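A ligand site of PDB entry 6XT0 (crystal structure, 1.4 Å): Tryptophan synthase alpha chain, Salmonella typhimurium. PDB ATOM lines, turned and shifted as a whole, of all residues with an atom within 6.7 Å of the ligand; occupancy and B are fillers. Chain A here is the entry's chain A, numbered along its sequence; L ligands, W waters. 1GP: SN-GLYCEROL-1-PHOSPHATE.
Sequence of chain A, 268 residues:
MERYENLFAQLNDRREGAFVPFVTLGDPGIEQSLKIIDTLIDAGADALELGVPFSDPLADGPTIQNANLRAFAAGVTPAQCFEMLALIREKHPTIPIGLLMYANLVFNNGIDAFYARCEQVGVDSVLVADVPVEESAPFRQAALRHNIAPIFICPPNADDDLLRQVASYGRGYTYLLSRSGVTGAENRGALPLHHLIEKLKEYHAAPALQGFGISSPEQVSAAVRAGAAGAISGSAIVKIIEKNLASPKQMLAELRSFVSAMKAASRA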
ATOM      1  N   PHE A  22     -30.134 -21.490  29.457  1.00  0.00           N
ATOM      2  CA  PHE A  22     -29.584 -20.677  30.536  1.00  0.00           C
ATOM      3  C   PHE A  22     -29.518 -19.227  30.077  1.00  0.00           C
ATOM      4  O   PHE A  22     -29.079 -18.942  28.961  1.00  0.00           O
ATOM      5  CB  PHE A  22     -28.173 -21.154  30.936  1.00  0.00           C
ATOM      6  CG  PHE A  22     -27.424 -20.173  31.814  1.00  0.00           C
ATOM      7  CD1 PHE A  22     -26.761 -19.095  31.262  1.00  0.00           C
ATOM      8  CD2 PHE A  22     -27.412 -20.324  33.194  1.00  0.00           C
ATOM      9  CE1 PHE A  22     -26.102 -18.172  32.065  1.00  0.00           C
ATOM     10  CE2 PHE A  22     -26.756 -19.414  34.000  1.00  0.00           C
ATOM     11  CZ  PHE A  22     -26.093 -18.346  33.438  1.00  0.00           C
ATOM     12  N   GLU A  49     -32.372 -22.743  33.602  1.00  0.00           N
ATOM     13  CA  GLU A  49     -31.191 -22.519  34.431  1.00  0.00           C
ATOM     14  C   GLU A  49     -30.919 -21.022  34.409  1.00  0.00           C
ATOM     15  O   GLU A  49     -30.864 -20.408  33.343  1.00  0.00           O
ATOM     16  CB  GLU A  49     -29.985 -23.295  33.908  1.00  0.00           C
ATOM     17  CG  GLU A  49     -30.083 -24.798  34.122  1.00  0.00           C
ATOM     18  CD  GLU A  49     -30.162 -25.149  35.587  1.00  0.00           C
ATOM     19  OE1 GLU A  49     -29.534 -24.445  36.409  1.00  0.00           O
ATOM     20  OE2 GLU A  49     -30.863 -26.129  35.926  1.00  0.00           O
ATOM     21  N   ASP A  60     -16.949 -19.271  33.801  1.00  0.00           N
ATOM     22  CA  ASP A  60     -17.598 -18.742  32.600  1.00  0.00           C
ATOM     23  C   ASP A  60     -16.585 -18.107  31.655  1.00  0.00           C
ATOM     24  O   ASP A  60     -15.616 -17.473  32.095  1.00  0.00           O
ATOM     25  CB  ASP A  60     -18.656 -17.714  32.985  1.00  0.00           C
ATOM     26  CG  ASP A  60     -19.908 -18.366  33.497  1.00  0.00           C
ATOM     27  OD1 ASP A  60     -20.449 -19.214  32.770  1.00  0.00           O
ATOM     28  OD2 ASP A  60     -20.315 -18.052  34.637  1.00  0.00           O
ATOM     29  N   THR A  63     -18.548 -14.809  26.927  1.00  0.00           N
ATOM     30  CA  THR A  63     -19.945 -14.533  26.615  1.00  0.00           C
ATOM     31  C   THR A  63     -20.753 -14.281  27.875  1.00  0.00           C
ATOM     32  O   THR A  63     -21.472 -13.279  27.992  1.00  0.00           O
ATOM     33  CB  THR A  63     -20.530 -15.696  25.814  1.00  0.00           C
ATOM     34  OG1 THR A  63     -19.925 -15.732  24.525  1.00  0.00           O
ATOM     35  CG2 THR A  63     -22.042 -15.543  25.671  1.00  0.00           C
ATOM     36  N   ILE A  64     -20.649 -15.185  28.857  1.00  0.00           N
ATOM     37  CA  ILE A  64     -21.439 -15.035  30.077  1.00  0.00           C
ATOM     38  C   ILE A  64     -20.792 -14.041  31.030  1.00  0.00           C
ATOM     39  O   ILE A  64     -21.496 -13.372  31.801  1.00  0.00           O
ATOM     40  CB  ILE A  64     -21.731 -16.412  30.688  1.00  0.00           C
ATOM     41  CG1 ILE A  64     -22.659 -17.189  29.751  1.00  0.00           C
ATOM     42  CG2 ILE A  64     -22.357 -16.265  32.078  1.00  0.00           C
ATOM     43  CD1 ILE A  64     -22.987 -18.609  30.178  1.00  0.00           C
ATOM     44  N   LEU A 100     -27.862 -21.264  38.941  1.00  0.00           N
ATOM     45  CA  LEU A 100     -26.428 -21.498  38.842  1.00  0.00           C
ATOM     46  C   LEU A 100     -25.763 -20.360  39.622  1.00  0.00           C
ATOM     47  O   LEU A 100     -25.849 -19.194  39.204  1.00  0.00           O
ATOM     48  CB  LEU A 100     -25.973 -21.508  37.399  1.00  0.00           C
ATOM     49  CG  LEU A 100     -26.591 -22.571  36.482  1.00  0.00           C
ATOM     50  CD1 LEU A 100     -25.897 -22.541  35.131  1.00  0.00           C
ATOM     51  CD2 LEU A 100     -26.493 -23.951  37.108  1.00  0.00           C
ATOM     52  N   LEU A 127     -27.167 -25.213  41.807  1.00  0.00           N
ATOM     53  CA  LEU A 127     -25.830 -25.721  41.537  1.00  0.00           C
ATOM     54  C   LEU A 127     -24.846 -24.617  41.891  1.00  0.00           C
ATOM     55  O   LEU A 127     -24.944 -23.509  41.353  1.00  0.00           O
ATOM     56  CB  LEU A 127     -25.682 -26.080  40.052  1.00  0.00           C
ATOM     57  CG  LEU A 127     -24.425 -26.797  39.586  1.00  0.00           C
ATOM     58  CD1 LEU A 127     -24.585 -27.263  38.138  1.00  0.00           C
ATOM     59  CD2 LEU A 127     -23.198 -25.915  39.683  1.00  0.00           C
ATOM     60  N   TYR A 173     -31.545 -33.211  38.954  1.00  0.00           N
ATOM     61  CA  TYR A 173     -30.832 -33.667  37.762  1.00  0.00           C
ATOM     62  C   TYR A 173     -29.354 -33.724  38.082  1.00  0.00           C
ATOM     63  O   TYR A 173     -28.896 -33.164  39.077  1.00  0.00           O
ATOM     64  CB  TYR A 173     -31.082 -32.732  36.561  1.00  0.00           C
ATOM     65  CG  TYR A 173     -30.433 -31.374  36.649  1.00  0.00           C
ATOM     66  CD1 TYR A 173     -31.081 -30.308  37.274  1.00  0.00           C
ATOM     67  CD2 TYR A 173     -29.179 -31.152  36.102  1.00  0.00           C
ATOM     68  CE1 TYR A 173     -30.475 -29.063  37.357  1.00  0.00           C
ATOM     69  CE2 TYR A 173     -28.580 -29.914  36.182  1.00  0.00           C
ATOM     70  CZ  TYR A 173     -29.220 -28.880  36.800  1.00  0.00           C
ATOM     71  OH  TYR A 173     -28.592 -27.650  36.865  1.00  0.00           O
ATOM     72  N   TYR A 175     -25.637 -32.763  36.494  1.00  0.00           N
ATOM     73  CA  TYR A 175     -25.044 -31.893  35.476  1.00  0.00           C
ATOM     74  C   TYR A 175     -23.867 -32.632  34.849  1.00  0.00           C
ATOM     75  O   TYR A 175     -22.812 -32.788  35.484  1.00  0.00           O
ATOM     76  CB  TYR A 175     -24.614 -30.553  36.074  1.00  0.00           C
ATOM     77  CG  TYR A 175     -24.373 -29.503  35.003  1.00  0.00           C
ATOM     78  CD1 TYR A 175     -23.344 -29.656  34.077  1.00  0.00           C
ATOM     79  CD2 TYR A 175     -25.171 -28.365  34.912  1.00  0.00           C
ATOM     80  CE1 TYR A 175     -23.110 -28.705  33.104  1.00  0.00           C
ATOM     81  CE2 TYR A 175     -24.942 -27.407  33.933  1.00  0.00           C
ATOM     82  CZ  TYR A 175     -23.919 -27.591  33.028  1.00  0.00           C
ATOM     83  OH  TYR A 175     -23.670 -26.656  32.060  1.00  0.00           O
ATOM     84  N   ARG A 179     -17.239 -31.253  28.570  1.00  0.00           N
ATOM     85  CA  ARG A 179     -15.812 -31.078  28.336  1.00  0.00           C
ATOM     86  C   ARG A 179     -15.230 -30.299  29.505  1.00  0.00           C
ATOM     87  O   ARG A 179     -15.952 -29.731  30.328  1.00  0.00           O
ATOM     88  CB  ARG A 179     -15.563 -30.295  27.040  1.00  0.00           C
ATOM     89  CG  ARG A 179     -16.279 -28.956  27.004  1.00  0.00           C
ATOM     90  CD  ARG A 179     -15.630 -27.940  26.067  1.00  0.00           C
ATOM     91  NE  ARG A 179     -16.434 -26.734  25.921  1.00  0.00           N
ATOM     92  CZ  ARG A 179     -16.522 -25.758  26.834  1.00  0.00           C
ATOM     93  NH1 ARG A 179     -15.839 -25.844  27.973  1.00  0.00           N
ATOM     94  NH2 ARG A 179     -17.278 -24.709  26.600  1.00  0.00           N
ATOM     95  N   VAL A 182     -14.175 -23.702  30.456  1.00  0.00           N
ATOM     96  CA  VAL A 182     -15.234 -22.843  30.957  1.00  0.00           C
ATOM     97  C   VAL A 182     -16.366 -22.787  29.928  1.00  0.00           C
ATOM     98  O   VAL A 182     -16.259 -23.318  28.834  1.00  0.00           O
ATOM     99  CB  VAL A 182     -14.722 -21.434  31.301  1.00  0.00           C
ATOM    100  CG1 VAL A 182     -13.708 -21.489  32.437  1.00  0.00           C
ATOM    101  CG2 VAL A 182     -14.109 -20.776  30.074  1.00  0.00           C
ATOM    102  N   THR A 183     -17.466 -22.115  30.309  1.00  0.00           N
ATOM    103  CA  THR A 183     -18.590 -21.994  29.394  1.00  0.00           C
ATOM    104  C   THR A 183     -18.166 -21.283  28.118  1.00  0.00           C
ATOM    105  O   THR A 183     -17.301 -20.408  28.119  1.00  0.00           O
ATOM    106  CB  THR A 183     -19.759 -21.237  30.034  1.00  0.00           C
ATOM    107  OG1 THR A 183     -19.373 -19.885  30.314  1.00  0.00           O
ATOM    108  CG2 THR A 183     -20.236 -21.934  31.330  1.00  0.00           C
ATOM    109  N   GLY A 184     -18.799 -21.683  27.016  1.00  0.00           N
ATOM    110  CA  GLY A 184     -18.406 -21.175  25.713  1.00  0.00           C
ATOM    111  C   GLY A 184     -19.097 -21.915  24.603  1.00  0.00           C
ATOM    112  O   GLY A 184     -18.982 -23.149  24.498  1.00  0.00           O
ATOM    113  N   ALA A 185     -19.820 -21.172  23.753  1.00  0.00           N
ATOM    114  CA  ALA A 185     -20.560 -21.788  22.664  1.00  0.00           C
ATOM    115  C   ALA A 185     -19.640 -22.236  21.539  1.00  0.00           C
ATOM    116  O   ALA A 185     -19.981 -23.164  20.788  1.00  0.00           O
ATOM    117  CB  ALA A 185     -21.595 -20.792  22.124  1.00  0.00           C
ATOM    118  N   GLU A 186     -18.484 -21.598  21.395  1.00  0.00           N
ATOM    119  CA  GLU A 186     -17.569 -21.929  20.315  1.00  0.00           C
ATOM    120  C   GLU A 186     -16.757 -23.189  20.594  1.00  0.00           C
ATOM    121  O   GLU A 186     -16.258 -23.815  19.645  1.00  0.00           O
ATOM    122  CB  GLU A 186     -16.608 -20.763  20.043  1.00  0.00           C
ATOM    123  CG  GLU A 186     -17.294 -19.489  19.552  1.00  0.00           C
ATOM    124  CD  GLU A 186     -18.069 -18.768  20.647  1.00  0.00           C
ATOM    125  OE1 GLU A 186     -17.913 -19.145  21.840  1.00  0.00           O
ATOM    126  OE2 GLU A 186     -18.829 -17.838  20.321  1.00  0.00           O
ATOM    127  N   ASN A 187     -16.618 -23.574  21.858  1.00  0.00           N
ATOM    128  CA  ASN A 187     -15.867 -24.760  22.247  1.00  0.00           C
ATOM    129  C   ASN A 187     -16.867 -25.893  22.450  1.00  0.00           C
ATOM    130  O   ASN A 187     -17.547 -25.974  23.472  1.00  0.00           O
ATOM    131  CB  ASN A 187     -15.080 -24.484  23.529  1.00  0.00           C
ATOM    132  CG  ASN A 187     -14.194 -25.648  23.937  1.00  0.00           C
ATOM    133  OD1 ASN A 187     -14.130 -26.665  23.245  1.00  0.00           O
ATOM    134  ND2 ASN A 187     -13.501 -25.495  25.059  1.00  0.00           N
ATOM    135  N   GLY A 211     -24.240 -30.247  29.605  1.00  0.00           N
ATOM    136  CA  GLY A 211     -24.028 -28.819  29.456  1.00  0.00           C
ATOM    137  C   GLY A 211     -22.571 -28.478  29.196  1.00  0.00           C
ATOM    138  O   GLY A 211     -21.660 -29.223  29.556  1.00  0.00           O
ATOM    139  N   PHE A 212     -22.386 -27.279  28.608  1.00  0.00           N
ATOM    140  CA  PHE A 212     -21.114 -26.709  28.155  1.00  0.00           C
ATOM    141  C   PHE A 212     -20.951 -26.964  26.655  1.00  0.00           C
ATOM    142  O   PHE A 212     -20.882 -28.122  26.221  1.00  0.00           O
ATOM    143  CB  PHE A 212     -19.879 -27.206  28.915  1.00  0.00           C
ATOM    144  CG  PHE A 212     -19.611 -26.478  30.216  1.00  0.00           C
ATOM    145  CD1 PHE A 212     -20.646 -26.151  31.070  1.00  0.00           C
ATOM    146  CD2 PHE A 212     -18.318 -26.153  30.590  1.00  0.00           C
ATOM    147  CE1 PHE A 212     -20.399 -25.496  32.275  1.00  0.00           C
ATOM    148  CE2 PHE A 212     -18.064 -25.501  31.788  1.00  0.00           C
ATOM    149  CZ  PHE A 212     -19.110 -25.171  32.620  1.00  0.00           C
ATOM    150  N   GLY A 213     -20.894 -25.899  25.872  1.00  0.00           N
ATOM    151  CA  GLY A 213     -20.612 -26.011  24.451  1.00  0.00           C
ATOM    152  C   GLY A 213     -21.772 -26.440  23.584  1.00  0.00           C
ATOM    153  O   GLY A 213     -21.578 -26.596  22.363  1.00  0.00           O
ATOM    154  N   ILE A 214     -22.961 -26.645  24.149  1.00  0.00           N
ATOM    155  CA  ILE A 214     -24.116 -27.091  23.359  1.00  0.00           C
ATOM    156  C   ILE A 214     -24.697 -25.871  22.665  1.00  0.00           C
ATOM    157  O   ILE A 214     -25.323 -25.017  23.309  1.00  0.00           O
ATOM    158  CB  ILE A 214     -25.167 -27.781  24.241  1.00  0.00           C
ATOM    159  CG1 ILE A 214     -24.562 -28.964  25.006  1.00  0.00           C
ATOM    160  CG2 ILE A 214     -26.350 -28.238  23.394  1.00  0.00           C
ATOM    161  CD1 ILE A 214     -24.119 -30.096  24.152  1.00  0.00           C
ATOM    162  N   SER A 215     -24.531 -25.797  21.348  1.00  0.00           N
ATOM    163  CA  SER A 215     -24.920 -24.601  20.615  1.00  0.00           C
ATOM    164  C   SER A 215     -25.720 -24.875  19.362  1.00  0.00           C
ATOM    165  O   SER A 215     -26.105 -23.926  18.673  1.00  0.00           O
ATOM    166  CB  SER A 215     -23.673 -23.784  20.249  1.00  0.00           C
ATOM    167  OG  SER A 215     -22.879 -23.555  21.408  1.00  0.00           O
ATOM    168  N   ILE A 232     -28.468 -28.622  28.165  1.00  0.00           N
ATOM    169  CA  ILE A 232     -28.485 -27.237  28.621  1.00  0.00           C
ATOM    170  C   ILE A 232     -27.699 -26.408  27.610  1.00  0.00           C
ATOM    171  O   ILE A 232     -26.631 -26.837  27.151  1.00  0.00           O
ATOM    172  CB  ILE A 232     -27.828 -27.134  30.013  1.00  0.00           C
ATOM    173  CG1 ILE A 232     -28.668 -27.870  31.066  1.00  0.00           C
ATOM    174  CG2 ILE A 232     -27.627 -25.669  30.424  1.00  0.00           C
ATOM    175  CD1 ILE A 232     -27.899 -28.170  32.340  1.00  0.00           C
ATOM    176  N   SER A 233     -28.207 -25.216  27.276  1.00  0.00           N
ATOM    177  CA  SER A 233     -27.510 -24.300  26.375  1.00  0.00           C
ATOM    178  C   SER A 233     -27.572 -22.890  26.959  1.00  0.00           C
ATOM    179  O   SER A 233     -28.675 -22.357  27.177  1.00  0.00           O
ATOM    180  CB  SER A 233     -28.150 -24.318  24.978  1.00  0.00           C
ATOM    181  OG  SER A 233     -27.502 -23.410  24.107  1.00  0.00           O
ATOM    182  N   GLY A 234     -26.399 -22.277  27.156  1.00  0.00           N
ATOM    183  CA  GLY A 234     -26.310 -20.954  27.745  1.00  0.00           C
ATOM    184  C   GLY A 234     -25.688 -19.916  26.818  1.00  0.00           C
ATOM    185  O   GLY A 234     -26.390 -19.024  26.326  1.00  0.00           O
ATOM    186  N   SER A 235     -24.393 -20.046  26.556  1.00  0.00           N
ATOM    187  CA  SER A 235     -23.685 -19.049  25.752  1.00  0.00           C
ATOM    188  C   SER A 235     -24.354 -18.829  24.400  1.00  0.00           C
ATOM    189  O   SER A 235     -24.452 -17.689  23.930  1.00  0.00           O
ATOM    190  CB  SER A 235     -22.230 -19.471  25.568  1.00  0.00           C
ATOM    191  OG  SER A 235     -21.550 -19.448  26.809  1.00  0.00           O
ATOM    192  N   ALA A 236     -24.821 -19.903  23.752  1.00  0.00           N
ATOM    193  CA  ALA A 236     -25.507 -19.735  22.473  1.00  0.00           C
ATOM    194  C   ALA A 236     -26.738 -18.841  22.614  1.00  0.00           C
ATOM    195  O   ALA A 236     -27.032 -18.038  21.734  1.00  0.00           O
ATOM    196  CB  ALA A 236     -25.905 -21.087  21.905  1.00  0.00           C
ATOM    197  N   ILE A 237     -27.481 -19.004  23.711  1.00  0.00           N
ATOM    198  CA  ILE A 237     -28.632 -18.157  23.972  1.00  0.00           C
ATOM    199  C   ILE A 237     -28.171 -16.730  24.244  1.00  0.00           C
ATOM    200  O   ILE A 237     -28.732 -15.758  23.713  1.00  0.00           O
ATOM    201  CB  ILE A 237     -29.428 -18.705  25.175  1.00  0.00           C
ATOM    202  CG1 ILE A 237     -29.979 -20.114  24.892  1.00  0.00           C
ATOM    203  CG2 ILE A 237     -30.564 -17.742  25.549  1.00  0.00           C
ATOM    204  CD1 ILE A 237     -31.329 -20.127  24.236  1.00  0.00           C
HETATM  205  C3  1GP L   1     -24.957 -23.155  31.883  1.00  0.00           C
HETATM  206  O3  1GP L   1     -23.740 -21.610  30.554  1.00  0.00           O
HETATM  207  C2  1GP L   1     -23.754 -22.964  30.963  1.00  0.00           C
HETATM  208  O2  1GP L   1     -24.707 -24.242  32.757  1.00  0.00           O
HETATM  209  C1  1GP L   1     -23.842 -23.875  29.741  1.00  0.00           C
HETATM  210  O1P 1GP L   1     -22.602 -23.809  29.071  1.00  0.00           O
HETATM  211  O2P 1GP L   1     -21.156 -23.395  27.051  1.00  0.00           O
HETATM  212  O3P 1GP L   1     -23.670 -23.403  26.819  1.00  0.00           O
HETATM  213  O4P 1GP L   1     -22.528 -21.543  27.977  1.00  0.00           O
HETATM  214  P   1GP L   1     -22.471 -23.028  27.697  1.00  0.00           P
HETATM  215  O   HOH W   1     -22.874 -20.438  33.362  1.00  0.00           O
HETATM  216  O   HOH W   2     -23.905 -22.519  24.217  1.00  0.00           O
HETATM  217  O   HOH W   3     -22.655 -23.056  34.434  1.00  0.00           O
HETATM  218  O   HOH W   4     -23.934 -25.961  26.853  1.00  0.00           O
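O of Gly 213 is in hydrogen-bond range of OG of Ser 215 (3.4 Å). O of Gly 184 sits at hydrogen-bond distance from NH2 of Arg 179 (3.1 Å). OD1 of Asp 60 is in hydrogen-bond range of OG1 of Thr 183, 2.8 Å away. The backbone NH (N) of Phe 22 sits at hydrogen-bond distance from the backbone carbonyl oxygen (O) of Ser 233 (2.8 Å). OG of Ser 233 lies within hydrogen-bond range of O of Ile 214 (2.8 Å).
Residues that only touch the ligand: Phe 22, Ile 64, Leu 100, Thr 183, Phe 212, Ile 232 and Ser 233. Of the 27 residues printed, 12 come within 4 Å of the ligand. Along chain A the residues within 4 Å of the ligand span positions 22 to 235. The nearest printed residue that does not touch the ligand is Arg 179 (4.1 Å).
Water W2 lies within hydrogen-bond range of an oxygen (O3P) of the ligand, the backbone NH (N) of Ala 236, the backbone carbonyl oxygen (O) of Ile 214, the side-chain hydroxyl (OG) of Ser 215 and the backbone NH (N) of Ser 235. Water W1 lies within hydrogen-bond range of the side-chain carboxylate of Asp 60 (2.8 Å) and an oxygen (O3) of the ligand (3.2 Å).
The backbone NH (N) of Ser 235 lies within hydrogen-bond range of an oxygen (O4P) of the ligand (2.8 Å). The side-chain hydroxyl of Ser 235 is in hydrogen-bond range of an oxygen (O4P) of the ligand (2.6 Å). An oxygen (O2) of the ligand is in hydrogen-bond range of the side-chain hydroxyl of Tyr 175 (2.7 Å). The backbone NH (N) of Gly 213 lies within hydrogen-bond range of an oxygen (O2P) of the ligand (2.8 Å). The backbone NH of Gly 184 lies within hydrogen-bond range of an oxygen (O2P) of the ligand, 2.9 Å away. The backbone NH (N) of Gly 234 is in hydrogen-bond range of an oxygen (O3P) of the ligand, 3.0 Å away.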
